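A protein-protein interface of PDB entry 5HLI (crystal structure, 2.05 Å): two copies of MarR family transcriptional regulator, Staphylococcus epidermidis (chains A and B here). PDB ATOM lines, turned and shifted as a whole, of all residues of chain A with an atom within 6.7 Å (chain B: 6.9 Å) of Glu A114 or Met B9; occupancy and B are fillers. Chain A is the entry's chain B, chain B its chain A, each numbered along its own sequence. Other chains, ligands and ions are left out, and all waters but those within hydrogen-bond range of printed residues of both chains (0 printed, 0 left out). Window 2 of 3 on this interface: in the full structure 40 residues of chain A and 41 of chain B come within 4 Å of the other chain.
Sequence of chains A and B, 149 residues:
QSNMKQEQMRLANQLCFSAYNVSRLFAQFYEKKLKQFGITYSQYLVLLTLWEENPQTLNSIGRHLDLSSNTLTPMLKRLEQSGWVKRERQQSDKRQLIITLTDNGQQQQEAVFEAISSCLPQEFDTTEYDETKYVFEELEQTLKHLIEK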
ATOM      1  N   LYS A  33       0.837 -18.326 -30.244  1.00  0.00           N
ATOM      2  CA  LYS A  33       0.838 -17.159 -29.371  1.00  0.00           C
ATOM      3  C   LYS A  33       0.122 -17.387 -28.044  1.00  0.00           C
ATOM      4  O   LYS A  33       0.429 -16.690 -27.070  1.00  0.00           O
ATOM      5  CB  LYS A  33       0.216 -15.958 -30.090  1.00  0.00           C
ATOM      6  CG  LYS A  33       0.945 -15.538 -31.365  1.00  0.00           C
ATOM      7  CD  LYS A  33       2.448 -15.377 -31.145  1.00  0.00           C
ATOM      8  CE  LYS A  33       2.775 -14.270 -30.143  1.00  0.00           C
ATOM      9  NZ  LYS A  33       2.658 -12.906 -30.733  1.00  0.00           N
ATOM     10  N   GLN A  36       1.943 -19.567 -24.288  1.00  0.00           N
ATOM     11  CA  GLN A  36       2.516 -18.975 -23.083  1.00  0.00           C
ATOM     12  C   GLN A  36       1.491 -18.811 -21.968  1.00  0.00           C
ATOM     13  O   GLN A  36       1.877 -18.707 -20.798  1.00  0.00           O
ATOM     14  CB  GLN A  36       3.133 -17.617 -23.417  1.00  0.00           C
ATOM     15  CG  GLN A  36       2.142 -16.639 -24.019  1.00  0.00           C
ATOM     16  CD  GLN A  36       2.787 -15.343 -24.456  1.00  0.00           C
ATOM     17  OE1 GLN A  36       3.547 -14.729 -23.706  1.00  0.00           O
ATOM     18  NE2 GLN A  36       2.490 -14.919 -25.679  1.00  0.00           N
ATOM     19  N   GLN A 109      -5.292  -9.277 -19.184  1.00  0.00           N
ATOM     20  CA  GLN A 109      -5.958  -8.969 -20.446  1.00  0.00           C
ATOM     21  C   GLN A 109      -5.014  -8.279 -21.423  1.00  0.00           C
ATOM     22  O   GLN A 109      -4.981  -8.619 -22.612  1.00  0.00           O
ATOM     23  CB  GLN A 109      -7.190  -8.100 -20.201  1.00  0.00           C
ATOM     24  CG  GLN A 109      -7.796  -7.540 -21.480  1.00  0.00           C
ATOM     25  CD  GLN A 109      -9.023  -6.683 -21.236  1.00  0.00           C
ATOM     26  OE1 GLN A 109      -9.440  -6.482 -20.096  1.00  0.00           O
ATOM     27  NE2 GLN A 109      -9.608  -6.173 -22.313  1.00  0.00           N
ATOM     28  N   GLU A 110      -4.230  -7.311 -20.940  1.00  0.00           N
ATOM     29  CA  GLU A 110      -3.365  -6.551 -21.835  1.00  0.00           C
ATOM     30  C   GLU A 110      -2.266  -7.426 -22.428  1.00  0.00           C
ATOM     31  O   GLU A 110      -1.922  -7.283 -23.607  1.00  0.00           O
ATOM     32  CB  GLU A 110      -2.766  -5.356 -21.095  1.00  0.00           C
ATOM     33  CG  GLU A 110      -3.794  -4.317 -20.673  1.00  0.00           C
ATOM     34  N   ALA A 111      -1.707  -8.339 -21.629  1.00  0.00           N
ATOM     35  CA  ALA A 111      -0.659  -9.220 -22.136  1.00  0.00           C
ATOM     36  C   ALA A 111      -1.199 -10.165 -23.203  1.00  0.00           C
ATOM     37  O   ALA A 111      -0.528 -10.425 -24.208  1.00  0.00           O
ATOM     38  CB  ALA A 111      -0.031 -10.006 -20.987  1.00  0.00           C
ATOM     39  N   VAL A 112      -2.409 -10.690 -23.003  1.00  0.00           N
ATOM     40  CA  VAL A 112      -3.015 -11.556 -24.010  1.00  0.00           C
ATOM     41  C   VAL A 112      -3.314 -10.767 -25.278  1.00  0.00           C
ATOM     42  O   VAL A 112      -3.012 -11.211 -26.391  1.00  0.00           O
ATOM     43  CB  VAL A 112      -4.281 -12.228 -23.450  1.00  0.00           C
ATOM     44  CG1 VAL A 112      -5.035 -12.949 -24.562  1.00  0.00           C
ATOM     45  CG2 VAL A 112      -3.912 -13.193 -22.332  1.00  0.00           C
ATOM     46  N   PHE A 113      -3.910  -9.580 -25.126  1.00  0.00           N
ATOM     47  CA  PHE A 113      -4.207  -8.743 -26.285  1.00  0.00           C
ATOM     48  C   PHE A 113      -2.940  -8.395 -27.054  1.00  0.00           C
ATOM     49  O   PHE A 113      -2.936  -8.395 -28.290  1.00  0.00           O
ATOM     50  CB  PHE A 113      -4.927  -7.466 -25.846  1.00  0.00           C
ATOM     51  CG  PHE A 113      -6.420  -7.614 -25.733  1.00  0.00           C
ATOM     52  CD1 PHE A 113      -6.999  -8.857 -25.544  1.00  0.00           C
ATOM     53  CD2 PHE A 113      -7.243  -6.504 -25.830  1.00  0.00           C
ATOM     54  CE1 PHE A 113      -8.373  -8.988 -25.444  1.00  0.00           C
ATOM     55  CE2 PHE A 113      -8.617  -6.629 -25.733  1.00  0.00           C
ATOM     56  CZ  PHE A 113      -9.182  -7.872 -25.541  1.00  0.00           C
ATOM     57  N   GLU A 114      -1.852  -8.095 -26.338  1.00  0.00           N
ATOM     58  CA  GLU A 114      -0.606  -7.728 -27.002  1.00  0.00           C
ATOM     59  C   GLU A 114      -0.038  -8.899 -27.796  1.00  0.00           C
ATOM     60  O   GLU A 114       0.452  -8.715 -28.915  1.00  0.00           O
ATOM     61  CB  GLU A 114       0.408  -7.230 -25.969  1.00  0.00           C
ATOM     62  CG  GLU A 114       1.679  -6.626 -26.555  1.00  0.00           C
ATOM     63  CD  GLU A 114       2.737  -7.664 -26.886  1.00  0.00           C
ATOM     64  OE1 GLU A 114       3.628  -7.363 -27.709  1.00  0.00           O
ATOM     65  OE2 GLU A 114       2.681  -8.777 -26.321  1.00  0.00           O
ATOM     66  N   ALA A 115      -0.099 -10.110 -27.235  1.00  0.00           N
ATOM     67  CA  ALA A 115       0.433 -11.277 -27.929  1.00  0.00           C
ATOM     68  C   ALA A 115      -0.362 -11.595 -29.188  1.00  0.00           C
ATOM     69  O   ALA A 115       0.184 -12.164 -30.141  1.00  0.00           O
ATOM     70  CB  ALA A 115       0.443 -12.484 -26.992  1.00  0.00           C
ATOM     71  N   ILE A 116      -1.642 -11.233 -29.216  1.00  0.00           N
ATOM     72  CA  ILE A 116      -2.498 -11.563 -30.348  1.00  0.00           C
ATOM     73  C   ILE A 116      -2.557 -10.431 -31.374  1.00  0.00           C
ATOM     74  O   ILE A 116      -2.746 -10.691 -32.568  1.00  0.00           O
ATOM     75  CB  ILE A 116      -3.906 -11.926 -29.835  1.00  0.00           C
ATOM     76  CG1 ILE A 116      -3.834 -13.135 -28.899  1.00  0.00           C
ATOM     77  CG2 ILE A 116      -4.858 -12.204 -30.985  1.00  0.00           C
ATOM     78  CD1 ILE A 116      -3.170 -14.343 -29.516  1.00  0.00           C
ATOM     79  N   SER A 117      -2.366  -9.183 -30.939  1.00  0.00           N
ATOM     80  CA  SER A 117      -2.636  -8.030 -31.793  1.00  0.00           C
ATOM     81  C   SER A 117      -1.755  -7.982 -33.035  1.00  0.00           C
ATOM     82  O   SER A 117      -2.115  -7.310 -34.007  1.00  0.00           O
ATOM     83  CB  SER A 117      -2.462  -6.735 -30.998  1.00  0.00           C
ATOM     84  OG  SER A 117      -1.143  -6.627 -30.491  1.00  0.00           O
ATOM     85  N   SER A 118      -0.615  -8.676 -33.030  1.00  0.00           N
ATOM     86  CA  SER A 118       0.279  -8.653 -34.181  1.00  0.00           C
ATOM     87  C   SER A 118      -0.324  -9.307 -35.419  1.00  0.00           C
ATOM     88  O   SER A 118       0.268  -9.199 -36.498  1.00  0.00           O
ATOM     89  CB  SER A 118       1.604  -9.335 -33.833  1.00  0.00           C
ATOM     90  OG  SER A 118       1.400 -10.688 -33.468  1.00  0.00           O
ATOM     91  N   SER B   2      -0.583   6.092 -25.253  1.00  0.00           N
ATOM     92  CA  SER B   2      -0.845   4.905 -24.445  1.00  0.00           C
ATOM     93  C   SER B   2      -2.254   4.377 -24.684  1.00  0.00           C
ATOM     94  O   SER B   2      -2.442   3.220 -25.079  1.00  0.00           O
ATOM     95  CB  SER B   2      -0.630   5.227 -22.964  1.00  0.00           C
ATOM     96  OG  SER B   2      -1.582   6.169 -22.502  1.00  0.00           O
ATOM     97  N   MET B   4      -4.263   5.249 -27.013  1.00  0.00           N
ATOM     98  CA  MET B   4      -4.444   5.031 -28.441  1.00  0.00           C
ATOM     99  C   MET B   4      -3.973   3.640 -28.851  1.00  0.00           C
ATOM    100  O   MET B   4      -4.583   2.998 -29.706  1.00  0.00           O
ATOM    101  CB  MET B   4      -3.698   6.097 -29.244  1.00  0.00           C
ATOM    102  N   LYS B   5      -2.886   3.177 -28.241  1.00  0.00           N
ATOM    103  CA  LYS B   5      -2.349   1.859 -28.561  1.00  0.00           C
ATOM    104  C   LYS B   5      -3.217   0.749 -27.981  1.00  0.00           C
ATOM    105  O   LYS B   5      -3.381  -0.305 -28.604  1.00  0.00           O
ATOM    106  CB  LYS B   5      -0.912   1.738 -28.057  1.00  0.00           C
ATOM    107  CG  LYS B   5       0.106   2.499 -28.893  1.00  0.00           C
ATOM    108  N   GLN B   6      -3.782   0.964 -26.789  1.00  0.00           N
ATOM    109  CA  GLN B   6      -4.661  -0.042 -26.204  1.00  0.00           C
ATOM    110  C   GLN B   6      -5.970  -0.174 -26.971  1.00  0.00           C
ATOM    111  O   GLN B   6      -6.606  -1.232 -26.909  1.00  0.00           O
ATOM    112  CB  GLN B   6      -4.949   0.278 -24.736  1.00  0.00           C
ATOM    113  CG  GLN B   6      -6.098   1.250 -24.520  1.00  0.00           C
ATOM    114  CD  GLN B   6      -6.729   1.117 -23.148  1.00  0.00           C
ATOM    115  OE1 GLN B   6      -6.145   0.531 -22.236  1.00  0.00           O
ATOM    116  NE2 GLN B   6      -7.933   1.658 -22.997  1.00  0.00           N
ATOM    117  N   GLU B   7      -6.385   0.871 -27.691  1.00  0.00           N
ATOM    118  CA  GLU B   7      -7.585   0.774 -28.512  1.00  0.00           C
ATOM    119  C   GLU B   7      -7.302   0.041 -29.817  1.00  0.00           C
ATOM    120  O   GLU B   7      -8.112  -0.782 -30.258  1.00  0.00           O
ATOM    121  CB  GLU B   7      -8.150   2.169 -28.786  1.00  0.00           C
ATOM    122  CG  GLU B   7      -9.452   2.179 -29.582  1.00  0.00           C
ATOM    123  CD  GLU B   7     -10.656   1.719 -28.773  1.00  0.00           C
ATOM    124  OE1 GLU B   7     -10.492   1.357 -27.588  1.00  0.00           O
ATOM    125  OE2 GLU B   7     -11.774   1.718 -29.330  1.00  0.00           O
ATOM    126  N   GLN B   8      -6.158   0.329 -30.447  1.00  0.00           N
ATOM    127  CA  GLN B   8      -5.743  -0.447 -31.612  1.00  0.00           C
ATOM    128  C   GLN B   8      -5.530  -1.910 -31.243  1.00  0.00           C
ATOM    129  O   GLN B   8      -5.821  -2.808 -32.042  1.00  0.00           O
ATOM    130  CB  GLN B   8      -4.469   0.147 -32.212  1.00  0.00           C
ATOM    131  CG  GLN B   8      -4.700   1.011 -33.440  1.00  0.00           C
ATOM    132  CD  GLN B   8      -5.690   2.129 -33.186  1.00  0.00           C
ATOM    133  N   MET B   9      -5.023  -2.165 -30.036  1.00  0.00           N
ATOM    134  CA  MET B   9      -4.867  -3.537 -29.566  1.00  0.00           C
ATOM    135  C   MET B   9      -6.212  -4.251 -29.500  1.00  0.00           C
ATOM    136  O   MET B   9      -6.309  -5.441 -29.823  1.00  0.00           O
ATOM    137  CB  MET B   9      -4.196  -3.545 -28.193  1.00  0.00           C
ATOM    138  CG  MET B   9      -3.288  -4.732 -27.937  1.00  0.00           C
ATOM    139  SD  MET B   9      -1.566  -4.360 -28.315  1.00  0.00           S
ATOM    140  CE  MET B   9      -1.194  -3.159 -27.038  1.00  0.00           C
ATOM    141  N   ARG B  10      -7.261  -3.538 -29.084  1.00  0.00           N
ATOM    142  CA  ARG B  10      -8.570  -4.164 -28.924  1.00  0.00           C
ATOM    143  C   ARG B  10      -9.211  -4.453 -30.275  1.00  0.00           C
ATOM    144  O   ARG B  10      -9.756  -5.542 -30.494  1.00  0.00           O
ATOM    145  CB  ARG B  10      -9.478  -3.270 -28.076  1.00  0.00           C
ATOM    146  CG  ARG B  10     -10.800  -3.917 -27.694  1.00  0.00           C
ATOM    147  CD  ARG B  10     -11.698  -2.946 -26.944  1.00  0.00           C
ATOM    148  NE  ARG B  10     -12.072  -1.801 -27.768  1.00  0.00           N
ATOM    149  CZ  ARG B  10     -13.150  -1.761 -28.544  1.00  0.00           C
ATOM    150  NH1 ARG B  10     -13.966  -2.804 -28.603  1.00  0.00           N
ATOM    151  NH2 ARG B  10     -13.415  -0.677 -29.261  1.00  0.00           N
ATOM    152  N   LEU B  11      -9.133  -3.482 -31.179  1.00  0.00           N
ATOM    153  CA  LEU B  11      -9.668  -3.643 -32.525  1.00  0.00           C
ATOM    154  C   LEU B  11      -8.967  -4.787 -33.248  1.00  0.00           C
ATOM    155  O   LEU B  11      -9.597  -5.544 -33.986  1.00  0.00           O
ATOM    156  CB  LEU B  11      -9.515  -2.346 -33.321  1.00  0.00           C
ATOM    157  CG  LEU B  11     -10.202  -1.108 -32.740  1.00  0.00           C
ATOM    158  CD1 LEU B  11     -10.281   0.000 -33.779  1.00  0.00           C
ATOM    159  CD2 LEU B  11     -11.587  -1.459 -32.216  1.00  0.00           C
ATOM    160  N   ALA B  12      -7.661  -4.912 -33.030  1.00  0.00           N
ATOM    161  CA  ALA B  12      -6.886  -5.982 -33.650  1.00  0.00           C
ATOM    162  C   ALA B  12      -7.386  -7.347 -33.196  1.00  0.00           C
ATOM    163  O   ALA B  12      -7.604  -8.246 -34.018  1.00  0.00           O
ATOM    164  CB  ALA B  12      -5.402  -5.814 -33.323  1.00  0.00           C
ATOM    165  N   ASN B  13      -7.578  -7.520 -31.886  1.00  0.00           N
ATOM    166  CA  ASN B  13      -8.153  -8.761 -31.382  1.00  0.00           C
ATOM    167  C   ASN B  13      -9.570  -8.989 -31.887  1.00  0.00           C
ATOM    168  O   ASN B  13     -10.037 -10.132 -31.886  1.00  0.00           O
ATOM    169  CB  ASN B  13      -8.145  -8.770 -29.852  1.00  0.00           C
ATOM    170  CG  ASN B  13      -6.811  -9.195 -29.277  1.00  0.00           C
ATOM    171  OD1 ASN B  13      -6.688 -10.277 -28.699  1.00  0.00           O
ATOM    172  ND2 ASN B  13      -5.799  -8.349 -29.434  1.00  0.00           N
ATOM    173  N   GLN B  14     -10.265  -7.935 -32.320  1.00  0.00           N
ATOM    174  CA  GLN B  14     -11.639  -8.077 -32.789  1.00  0.00           C
ATOM    175  C   GLN B  14     -11.727  -8.298 -34.295  1.00  0.00           C
ATOM    176  O   GLN B  14     -12.527  -9.124 -34.747  1.00  0.00           O
ATOM    177  CB  GLN B  14     -12.465  -6.852 -32.390  1.00  0.00           C
ATOM    178  CG  GLN B  14     -12.892  -6.853 -30.931  1.00  0.00           C
ATOM    179  CD  GLN B  14     -13.859  -5.732 -30.603  1.00  0.00           C
ATOM    180  OE1 GLN B  14     -14.226  -4.939 -31.470  1.00  0.00           O
ATOM    181  NE2 GLN B  14     -14.285  -5.668 -29.347  1.00  0.00           N
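The side-chain sulfur of Met B9 sits at hydrogen-bond distance from the side-chain hydroxyl of Ser A117.
The side-chain amide nitrogen (ND2) of Asn B13 is in hydrogen-bond range of the backbone carbonyl oxygen (O) of Phe A113 (3.1 Å).
The side-chain carboxylate of Glu B7 lies within salt-bridge range of the guanidinium group of Arg B10 (2.9 Å).
The side-chain amide nitrogen of Asn B13 sits at hydrogen-bond distance from the backbone carbonyl oxygen of Met B9.
The guanidinium group (NH1) of Arg B10 sits close to the side-chain amide nitrogen (NE2) of Gln B14 (3.0 Å).
O of Phe A113 sits close to OG of Ser A117 (3.3 Å).
OG of Ser A117 is in hydrogen-bond range of O of Glu A114 (3.1 Å).
Among the printed residues, pairs that only touch across the chains: Ile A116 with Asn B13, Ser A117 with Ala B12, Phe A113 with Met B9, Glu A114 with Met B9, Ser A117 with Asn B13 and Phe A113 with Arg B10.
Of the printed residues of chain B, Phe A113 touches Met B9 (3.7 Å), Arg B10 (3.996 Å) and Asn B13 (3.1 Å).
Of chain B, only Met B9 comes within 4 Å of Glu A114.
Of the printed residues of chain B, Ile A116 touches Asn B13.
Met B9 touches just these residues of chain A: Phe A113, Glu A114 and Ser A117.
Printed residues of chain A within 4 Å of Arg B10: Phe A113.
Of the printed residues of chain A, Ala B12 touches Ser A117.
Printed residues of chain A within 4 Å of Asn B13: Phe A113, Ile A116 and Ser A117.
The nearest residue of chain A that does not touch Met B9 is Glu A110 (5.2 Å).
Printed residues of chain A that touch a printed residue of chain B: Phe A113, Glu A114, Ile A116 and Ser A117.
Of the 12 printed residues of chain B, 4 touch a printed residue of chain A.
Among the printed residues, 8 pairs touch across the chains.
No position is printed for both chains.
Of the 8 pairs that touch across the chains among the printed residues, none has its exchanged pair printed and touching as well.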
